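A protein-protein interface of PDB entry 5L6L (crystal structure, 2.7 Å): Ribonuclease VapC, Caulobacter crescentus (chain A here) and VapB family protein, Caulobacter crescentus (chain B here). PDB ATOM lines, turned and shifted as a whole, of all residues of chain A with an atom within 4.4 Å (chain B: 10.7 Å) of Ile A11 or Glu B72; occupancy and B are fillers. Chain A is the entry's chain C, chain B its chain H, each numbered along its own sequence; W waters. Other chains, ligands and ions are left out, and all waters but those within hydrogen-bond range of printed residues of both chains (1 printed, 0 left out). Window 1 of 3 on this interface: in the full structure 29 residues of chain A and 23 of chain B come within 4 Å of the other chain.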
ATOM      1  N   THR A   7      -0.454 -26.800  -1.140  1.00  0.00           N
ATOM      2  CA  THR A   7      -0.965 -26.158   0.070  1.00  0.00           C
ATOM      3  C   THR A   7      -1.138 -24.648  -0.104  1.00  0.00           C
ATOM      4  O   THR A   7      -2.062 -24.064   0.460  1.00  0.00           O
ATOM      5  CB  THR A   7      -0.014 -26.452   1.249  1.00  0.00           C
ATOM      6  OG1 THR A   7      -0.015 -27.851   1.542  1.00  0.00           O
ATOM      7  CG2 THR A   7      -0.412 -25.684   2.510  1.00  0.00           C
ATOM      8  N   ASN A   8      -0.264 -23.993  -0.875  1.00  0.00           N
ATOM      9  CA  ASN A   8      -0.427 -22.557  -1.087  1.00  0.00           C
ATOM     10  C   ASN A   8      -1.676 -22.256  -1.897  1.00  0.00           C
ATOM     11  O   ASN A   8      -2.420 -21.325  -1.565  1.00  0.00           O
ATOM     12  CB  ASN A   8       0.805 -21.969  -1.763  1.00  0.00           C
ATOM     13  CG  ASN A   8       1.895 -21.639  -0.770  1.00  0.00           C
ATOM     14  OD1 ASN A   8       1.675 -20.847   0.158  1.00  0.00           O
ATOM     15  ND2 ASN A   8       3.076 -22.263  -0.939  1.00  0.00           N
ATOM     16  N   VAL A   9      -1.930 -23.033  -2.955  1.00  0.00           N
ATOM     17  CA  VAL A   9      -3.201 -22.921  -3.663  1.00  0.00           C
ATOM     18  C   VAL A   9      -4.367 -23.027  -2.689  1.00  0.00           C
ATOM     19  O   VAL A   9      -5.313 -22.232  -2.741  1.00  0.00           O
ATOM     20  CB  VAL A   9      -3.294 -23.992  -4.757  1.00  0.00           C
ATOM     21  CG1 VAL A   9      -4.687 -23.967  -5.400  1.00  0.00           C
ATOM     22  CG2 VAL A   9      -2.177 -23.810  -5.782  1.00  0.00           C
ATOM     23  N   ALA A  10      -4.315 -23.998  -1.769  1.00  0.00           N
ATOM     24  CA  ALA A  10      -5.435 -24.185  -0.852  1.00  0.00           C
ATOM     25  C   ALA A  10      -5.510 -23.074   0.185  1.00  0.00           C
ATOM     26  O   ALA A  10      -6.605 -22.706   0.620  1.00  0.00           O
ATOM     27  CB  ALA A  10      -5.340 -25.544  -0.175  1.00  0.00           C
ATOM     28  N   ILE A  11      -4.373 -22.521   0.596  1.00  0.00           N
ATOM     29  CA  ILE A  11      -4.437 -21.375   1.494  1.00  0.00           C
ATOM     30  C   ILE A  11      -5.058 -20.190   0.772  1.00  0.00           C
ATOM     31  O   ILE A  11      -5.947 -19.517   1.310  1.00  0.00           O
ATOM     32  CB  ILE A  11      -3.047 -21.038   2.068  1.00  0.00           C
ATOM     33  CG1 ILE A  11      -2.517 -22.210   2.894  1.00  0.00           C
ATOM     34  CG2 ILE A  11      -3.108 -19.764   2.917  1.00  0.00           C
ATOM     35  CD1 ILE A  11      -1.153 -21.970   3.449  1.00  0.00           C
ATOM     36  N   HIS A  12      -4.643 -19.947  -0.475  1.00  0.00           N
ATOM     37  CA  HIS A  12      -5.245 -18.856  -1.237  1.00  0.00           C
ATOM     38  C   HIS A  12      -6.703 -19.136  -1.567  1.00  0.00           C
ATOM     39  O   HIS A  12      -7.502 -18.199  -1.685  1.00  0.00           O
ATOM     40  CB  HIS A  12      -4.439 -18.593  -2.502  1.00  0.00           C
ATOM     41  CG  HIS A  12      -3.122 -17.937  -2.226  1.00  0.00           C
ATOM     42  ND1 HIS A  12      -2.808 -16.672  -2.672  1.00  0.00           N
ATOM     43  CD2 HIS A  12      -2.060 -18.351  -1.493  1.00  0.00           C
ATOM     44  CE1 HIS A  12      -1.599 -16.345  -2.248  1.00  0.00           C
ATOM     45  NE2 HIS A  12      -1.127 -17.347  -1.528  1.00  0.00           N
ATOM     46  N   LEU A  13      -7.072 -20.404  -1.720  1.00  0.00           N
ATOM     47  CA  LEU A  13      -8.477 -20.711  -1.892  1.00  0.00           C
ATOM     48  C   LEU A  13      -9.242 -20.388  -0.616  1.00  0.00           C
ATOM     49  O   LEU A  13     -10.258 -19.690  -0.651  1.00  0.00           O
ATOM     50  CB  LEU A  13      -8.647 -22.175  -2.310  1.00  0.00           C
ATOM     51  CG  LEU A  13     -10.056 -22.654  -2.703  1.00  0.00           C
ATOM     52  CD1 LEU A  13     -10.635 -21.764  -3.795  1.00  0.00           C
ATOM     53  CD2 LEU A  13     -10.031 -24.104  -3.157  1.00  0.00           C
ATOM     54  N   ARG A  14      -8.737 -20.851   0.531  1.00  0.00           N
ATOM     55  CA  ARG A  14      -9.365 -20.537   1.812  1.00  0.00           C
ATOM     56  C   ARG A  14      -9.530 -19.028   2.003  1.00  0.00           C
ATOM     57  O   ARG A  14     -10.586 -18.562   2.442  1.00  0.00           O
ATOM     58  CB  ARG A  14      -8.546 -21.147   2.958  1.00  0.00           C
ATOM     59  CG  ARG A  14      -9.233 -21.072   4.339  1.00  0.00           C
ATOM     60  CD  ARG A  14      -8.293 -21.192   5.530  1.00  0.00           C
ATOM     61  NE  ARG A  14      -7.181 -20.275   5.377  1.00  0.00           N
ATOM     62  CZ  ARG A  14      -5.953 -20.472   5.852  1.00  0.00           C
ATOM     63  NH1 ARG A  14      -5.676 -21.570   6.538  1.00  0.00           N
ATOM     64  NH2 ARG A  14      -4.989 -19.568   5.627  1.00  0.00           N
ATOM     65  N   ASP A  15      -8.509 -18.243   1.675  1.00  0.00           N
ATOM     66  CA  ASP A  15      -8.518 -16.830   2.023  1.00  0.00           C
ATOM     67  C   ASP A  15      -9.013 -15.946   0.879  1.00  0.00           C
ATOM     68  O   ASP A  15      -8.816 -14.730   0.912  1.00  0.00           O
ATOM     69  CB  ASP A  15      -7.130 -16.397   2.504  1.00  0.00           C
ATOM     70  CG  ASP A  15      -6.746 -17.032   3.851  1.00  0.00           C
ATOM     71  OD1 ASP A  15      -7.504 -17.887   4.359  1.00  0.00           O
ATOM     72  OD2 ASP A  15      -5.676 -16.687   4.405  1.00  0.00           O
ATOM     73  N   LEU A  41      -3.762 -26.166   6.905  1.00  0.00           N
ATOM     74  CA  LEU A  41      -4.925 -25.295   6.862  1.00  0.00           C
ATOM     75  C   LEU A  41      -5.578 -25.190   8.234  1.00  0.00           C
ATOM     76  O   LEU A  41      -5.927 -24.084   8.667  1.00  0.00           O
ATOM     77  CB  LEU A  41      -5.910 -25.802   5.801  1.00  0.00           C
ATOM     78  CG  LEU A  41      -5.448 -25.748   4.331  1.00  0.00           C
ATOM     79  CD1 LEU A  41      -6.082 -26.827   3.509  1.00  0.00           C
ATOM     80  CD2 LEU A  41      -5.741 -24.403   3.736  1.00  0.00           C
ATOM     81  N   GLY A  44      -3.722 -22.753  10.343  1.00  0.00           N
ATOM     82  CA  GLY A  44      -3.862 -21.350   9.982  1.00  0.00           C
ATOM     83  C   GLY A  44      -5.101 -20.694  10.557  1.00  0.00           C
ATOM     84  O   GLY A  44      -5.074 -19.510  10.909  1.00  0.00           O
ATOM     85  N   ARG A  47      -4.472 -18.567  13.699  1.00  0.00           N
ATOM     86  CA  ARG A  47      -3.258 -17.777  13.910  1.00  0.00           C
ATOM     87  C   ARG A  47      -3.579 -16.300  14.180  1.00  0.00           C
ATOM     88  O   ARG A  47      -3.051 -15.715  15.132  1.00  0.00           O
ATOM     89  CB  ARG A  47      -2.295 -17.962  12.731  1.00  0.00           C
ATOM     90  CG  ARG A  47      -1.566 -19.330  12.777  1.00  0.00           C
ATOM     91  CD  ARG A  47      -0.622 -19.607  11.587  1.00  0.00           C
ATOM     92  NE  ARG A  47       0.292 -18.491  11.332  1.00  0.00           N
ATOM     93  CZ  ARG A  47       1.054 -18.351  10.243  1.00  0.00           C
ATOM     94  NH1 ARG A  47       1.046 -19.271   9.283  1.00  0.00           N
ATOM     95  NH2 ARG A  47       1.819 -17.272  10.109  1.00  0.00           N
ATOM     96  N   ARG A  55     -12.415 -18.094   7.614  1.00  0.00           N
ATOM     97  CA  ARG A  55     -11.306 -19.065   7.678  1.00  0.00           C
ATOM     98  C   ARG A  55     -11.727 -20.396   8.309  1.00  0.00           C
ATOM     99  O   ARG A  55     -11.612 -21.443   7.667  1.00  0.00           O
ATOM    100  CB  ARG A  55     -10.093 -18.530   8.458  1.00  0.00           C
ATOM    101  CG  ARG A  55      -9.203 -17.549   7.714  1.00  0.00           C
ATOM    102  CD  ARG A  55      -7.747 -17.686   8.115  1.00  0.00           C
ATOM    103  NE  ARG A  55      -6.893 -16.859   7.273  1.00  0.00           N
ATOM    104  CZ  ARG A  55      -6.186 -15.805   7.689  1.00  0.00           C
ATOM    105  NH1 ARG A  55      -5.457 -15.128   6.811  1.00  0.00           N
ATOM    106  NH2 ARG A  55      -6.191 -15.422   8.966  1.00  0.00           N
ATOM    107  N   LEU B  62     -18.074 -19.972  -1.633  1.00  0.00           N
ATOM    108  CA  LEU B  62     -16.821 -19.305  -1.260  1.00  0.00           C
ATOM    109  C   LEU B  62     -16.828 -17.823  -1.632  1.00  0.00           C
ATOM    110  O   LEU B  62     -16.607 -16.962  -0.778  1.00  0.00           O
ATOM    111  CB  LEU B  62     -15.608 -20.029  -1.850  1.00  0.00           C
ATOM    112  CG  LEU B  62     -14.564 -20.546  -0.823  1.00  0.00           C
ATOM    113  CD1 LEU B  62     -15.151 -21.176   0.444  1.00  0.00           C
ATOM    114  CD2 LEU B  62     -13.608 -21.529  -1.465  1.00  0.00           C
ATOM    115  N   PRO B  66     -17.533 -13.441   2.965  1.00  0.00           N
ATOM    116  CA  PRO B  66     -16.446 -12.486   3.109  1.00  0.00           C
ATOM    117  C   PRO B  66     -15.111 -13.204   3.001  1.00  0.00           C
ATOM    118  O   PRO B  66     -15.014 -14.416   3.203  1.00  0.00           O
ATOM    119  CB  PRO B  66     -16.672 -11.904   4.510  1.00  0.00           C
ATOM    120  CG  PRO B  66     -18.059 -12.150   4.807  1.00  0.00           C
ATOM    121  CD  PRO B  66     -18.406 -13.424   4.144  1.00  0.00           C
ATOM    122  N   ARG B  67     -14.085 -12.459   2.633  1.00  0.00           N
ATOM    123  CA  ARG B  67     -12.740 -13.011   2.650  1.00  0.00           C
ATOM    124  C   ARG B  67     -11.924 -12.364   3.764  1.00  0.00           C
ATOM    125  O   ARG B  67     -12.270 -11.285   4.256  1.00  0.00           O
ATOM    126  CB  ARG B  67     -12.037 -12.821   1.299  1.00  0.00           C
ATOM    127  CG  ARG B  67     -11.671 -11.400   0.984  1.00  0.00           C
ATOM    128  CD  ARG B  67     -11.063 -11.277  -0.405  1.00  0.00           C
ATOM    129  NE  ARG B  67     -11.951 -11.802  -1.443  1.00  0.00           N
ATOM    130  CZ  ARG B  67     -11.824 -11.537  -2.742  1.00  0.00           C
ATOM    131  NH1 ARG B  67     -10.846 -10.739  -3.168  1.00  0.00           N
ATOM    132  NH2 ARG B  67     -12.674 -12.066  -3.611  1.00  0.00           N
ATOM    133  N   PRO B  68     -10.870 -13.026   4.229  1.00  0.00           N
ATOM    134  CA  PRO B  68      -9.974 -12.388   5.202  1.00  0.00           C
ATOM    135  C   PRO B  68      -9.255 -11.188   4.591  1.00  0.00           C
ATOM    136  O   PRO B  68      -9.135 -11.064   3.369  1.00  0.00           O
ATOM    137  CB  PRO B  68      -8.989 -13.504   5.569  1.00  0.00           C
ATOM    138  CG  PRO B  68      -9.661 -14.769   5.167  1.00  0.00           C
ATOM    139  CD  PRO B  68     -10.567 -14.447   4.024  1.00  0.00           C
ATOM    140  N   ASP B  69      -8.788 -10.290   5.472  1.00  0.00           N
ATOM    141  CA  ASP B  69      -8.004  -9.120   5.061  1.00  0.00           C
ATOM    142  C   ASP B  69      -6.933  -9.486   4.039  1.00  0.00           C
ATOM    143  O   ASP B  69      -6.873  -8.921   2.936  1.00  0.00           O
ATOM    144  CB  ASP B  69      -7.320  -8.475   6.274  1.00  0.00           C
ATOM    145  CG  ASP B  69      -8.289  -7.838   7.237  1.00  0.00           C
ATOM    146  OD1 ASP B  69      -9.522  -7.983   7.053  1.00  0.00           O
ATOM    147  OD2 ASP B  69      -7.813  -7.212   8.209  1.00  0.00           O
ATOM    148  N   SER B  70      -6.055 -10.417   4.416  1.00  0.00           N
ATOM    149  CA  SER B  70      -4.918 -10.814   3.607  1.00  0.00           C
ATOM    150  C   SER B  70      -4.887 -12.331   3.505  1.00  0.00           C
ATOM    151  O   SER B  70      -5.568 -13.031   4.258  1.00  0.00           O
ATOM    152  CB  SER B  70      -3.616 -10.311   4.218  1.00  0.00           C
ATOM    153  OG  SER B  70      -3.465 -10.911   5.492  1.00  0.00           O
ATOM    154  N   VAL B  71      -4.091 -12.834   2.559  1.00  0.00           N
ATOM    155  CA  VAL B  71      -3.820 -14.268   2.469  1.00  0.00           C
ATOM    156  C   VAL B  71      -2.665 -14.606   3.399  1.00  0.00           C
ATOM    157  O   VAL B  71      -1.656 -13.891   3.444  1.00  0.00           O
ATOM    158  CB  VAL B  71      -3.508 -14.692   1.023  1.00  0.00           C
ATOM    159  CG1 VAL B  71      -3.223 -16.175   0.966  1.00  0.00           C
ATOM    160  CG2 VAL B  71      -4.655 -14.340   0.089  1.00  0.00           C
ATOM    161  N   GLU B  72      -2.835 -15.678   4.166  1.00  0.00           N
ATOM    162  CA  GLU B  72      -1.805 -16.176   5.057  1.00  0.00           C
ATOM    163  C   GLU B  72      -0.505 -16.432   4.305  1.00  0.00           C
ATOM    164  O   GLU B  72      -0.499 -16.849   3.147  1.00  0.00           O
ATOM    165  CB  GLU B  72      -2.300 -17.468   5.722  1.00  0.00           C
ATOM    166  CG  GLU B  72      -1.324 -18.152   6.688  1.00  0.00           C
ATOM    167  CD  GLU B  72      -1.900 -19.440   7.287  1.00  0.00           C
ATOM    168  OE1 GLU B  72      -1.419 -20.537   6.930  1.00  0.00           O
ATOM    169  OE2 GLU B  72      -2.849 -19.350   8.110  1.00  0.00           O
ATOM    170  N   ILE B  73       0.614 -16.177   4.971  1.00  0.00           N
ATOM    171  CA  ILE B  73       1.903 -16.653   4.491  1.00  0.00           C
ATOM    172  C   ILE B  73       2.152 -18.027   5.122  1.00  0.00           C
ATOM    173  O   ILE B  73       2.323 -18.148   6.341  1.00  0.00           O
ATOM    174  CB  ILE B  73       3.023 -15.659   4.809  1.00  0.00           C
ATOM    175  CG1 ILE B  73       2.707 -14.290   4.215  1.00  0.00           C
ATOM    176  CG2 ILE B  73       4.317 -16.126   4.228  1.00  0.00           C
ATOM    177  CD1 ILE B  73       3.581 -13.187   4.780  1.00  0.00           C
ATOM    178  N   ARG B  74       2.155 -19.064   4.283  1.00  0.00           N
ATOM    179  CA  ARG B  74       2.460 -20.422   4.710  1.00  0.00           C
ATOM    180  C   ARG B  74       3.697 -20.464   5.592  1.00  0.00           C
ATOM    181  O   ARG B  74       4.743 -19.923   5.234  1.00  0.00           O
ATOM    182  CB  ARG B  74       2.671 -21.310   3.485  1.00  0.00           C
ATOM    183  CG  ARG B  74       2.831 -22.771   3.811  1.00  0.00           C
ATOM    184  CD  ARG B  74       3.186 -23.579   2.572  1.00  0.00           C
ATOM    185  NE  ARG B  74       3.222 -25.004   2.868  1.00  0.00           N
ATOM    186  CZ  ARG B  74       3.584 -25.938   1.998  1.00  0.00           C
ATOM    187  NH1 ARG B  74       3.585 -27.222   2.344  1.00  0.00           N
ATOM    188  NH2 ARG B  74       3.934 -25.593   0.781  1.00  0.00           N
ATOM    189  N   ASP B  75       3.556 -21.078   6.757  1.00  0.00           N
ATOM    190  CA  ASP B  75       4.708 -21.378   7.600  1.00  0.00           C
ATOM    191  C   ASP B  75       5.503 -22.528   6.998  1.00  0.00           C
ATOM    192  O   ASP B  75       4.933 -23.553   6.609  1.00  0.00           O
ATOM    193  CB  ASP B  75       4.265 -21.747   9.014  1.00  0.00           C
ATOM    194  CG  ASP B  75       4.213 -20.563   9.946  1.00  0.00           C
ATOM    195  OD1 ASP B  75       4.759 -19.490   9.602  1.00  0.00           O
ATOM    196  OD2 ASP B  75       3.637 -20.716  11.042  1.00  0.00           O
ATOM    197  N   GLU B  76       6.814 -22.367   6.937  1.00  0.00           N
ATOM    198  CA  GLU B  76       7.696 -23.373   6.363  1.00  0.00           C
ATOM    199  C   GLU B  76       8.547 -23.999   7.466  1.00  0.00           C
ATOM    200  O   GLU B  76       8.431 -23.652   8.647  1.00  0.00           O
ATOM    201  CB  GLU B  76       8.543 -22.759   5.241  1.00  0.00           C
ATOM    202  CG  GLU B  76       8.184 -23.297   3.844  1.00  0.00           C
ATOM    203  CD  GLU B  76       7.437 -22.296   2.957  1.00  0.00           C
ATOM    204  OE1 GLU B  76       7.396 -21.094   3.285  1.00  0.00           O
ATOM    205  OE2 GLU B  76       6.881 -22.708   1.914  1.00  0.00           O
ATOM    206  N   LEU B  78       8.619 -26.999   8.891  1.00  0.00           N
ATOM    207  CA  LEU B  78       7.903 -27.655   9.976  1.00  0.00           C
ATOM    208  C   LEU B  78       8.657 -28.866  10.527  1.00  0.00           C
ATOM    209  O   LEU B  78       8.628 -29.110  11.741  1.00  0.00           O
ATOM    210  CB  LEU B  78       6.509 -28.057   9.504  1.00  0.00           C
ATOM    211  CG  LEU B  78       5.560 -26.940   9.089  1.00  0.00           C
ATOM    212  CD1 LEU B  78       4.179 -27.530   8.827  1.00  0.00           C
ATOM    213  CD2 LEU B  78       5.506 -25.800  10.106  1.00  0.00           C
HETATM  214  O   HOH W   1       2.151 -18.756   1.400  1.00  0.00           O
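O of Ser B70 sits at hydrogen-bond distance from NH1 of Arg A55 (3.3 Å).
The side-chain carboxylate of Asp B75 lies within salt-bridge range of the guanidinium group of Arg A47, at 3.4 Å.
The guanidinium group of Arg A14 is in salt-bridge range of the side-chain carboxylate of Glu B72 (3.3 Å).
The backbone NH of Glu B72 is in hydrogen-bond range of the side-chain carboxylate of Asp A15, 3.0 Å away.
The side-chain carboxylate of Glu B72 lies within salt-bridge range of the guanidinium group of Arg A47 (3.6 Å).
The backbone carbonyl oxygen (O) of Ile B73 sits at hydrogen-bond distance from the guanidinium group (NH1) of Arg A47, 3.4 Å away.
CB of Thr A7 touches CZ of Arg B74, 3.7 Å away.
Glu B72 touches Ile A11 (CB to CG2, 3.7 Å).
His A12 touches Val B71.
Leu B62 touches Leu A13 (CD2 to CD1, 3.8 Å).
CB of Arg B67 touches O of Asp A15 (3.8 Å).
O of Asp A15 touches CD of Pro B68, at 3.6 Å.
OD2 of Asp A15 touches O of Ser B70, at 3.7 Å.
Asp A15 touches Val B71.
Pro B68 touches Arg A55 (CG to CG, 3.8 Å).
Arg A55 touches Glu B72 (NH1 to N, 3.8 Å).
Of chain B, only Glu B72 (3.7 Å) and Arg B74 (3.9 Å) come within 4 Å of Ile A11.
Of chain A, only Ile A11, Arg A14, Asp A15, Gly A44, Arg A47 and Arg A55 come within 4 Å of Glu B72.
Printed residues of chain B within 4 Å of Thr A7: Arg B74 (3.7 Å).
Of chain B, only Arg B74 (3.5 Å) comes within 4 Å of Asn A8.
Of chain B, only Glu B72 comes within 4 Å of Arg A14.
Asp A15 touches just these residues of chain B: Arg B67, Pro B68, Ser B70, Val B71 and Glu B72.
Of the printed residues of chain A, Ile B73 touches Arg A47.
Of the printed residues of chain B, Arg A55 touches Pro B68 (3.8 Å), Ser B70 (3.3 Å) and Glu B72 (3.8 Å).
Of the printed residues of chain A, Pro B68 touches Asp A15 and Arg A55.
Asp B69 touches none of the printed residues of chain A.
The nearest residue of chain B that does not touch Ile A11 is Val B71 (4.1 Å).
The nearest printed residue of chain A that does not touch Glu B72 is His A12 (4.7 Å).
The nearest printed residue of chain B that does not touch Arg A47 is Arg B74 (4.7 Å).
Water W1 lies within hydrogen-bond range of OD1 of Asn A8 (2.5 Å) and N of Arg B74 (2.9 Å).
Of the 13 printed residues of chain B, 9 touch a printed residue of chain A.
Of the 13 printed residues of chain A, 10 touch a printed residue of chain B.
Printed residues of chain A that touch a printed residue of chain B: Thr A7, Asn A8, Ile A11, His A12, Leu A13, Arg A14, Asp A15, Gly A44, Arg A47 and Arg A55.
The side-chain carboxylate of Asp A15 lies within salt-bridge range of the guanidinium group of Arg A55 (2.9 Å).
The guanidinium group (NH1) of Arg A14 sits at hydrogen-bond distance from the backbone carbonyl oxygen (O) of Leu A41, at 3.3 Å.
The side-chain carboxylate (OD1) of Asp A15 lies within salt-bridge range of the guanidinium group (NE) of Arg A14 (2.6 Å).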
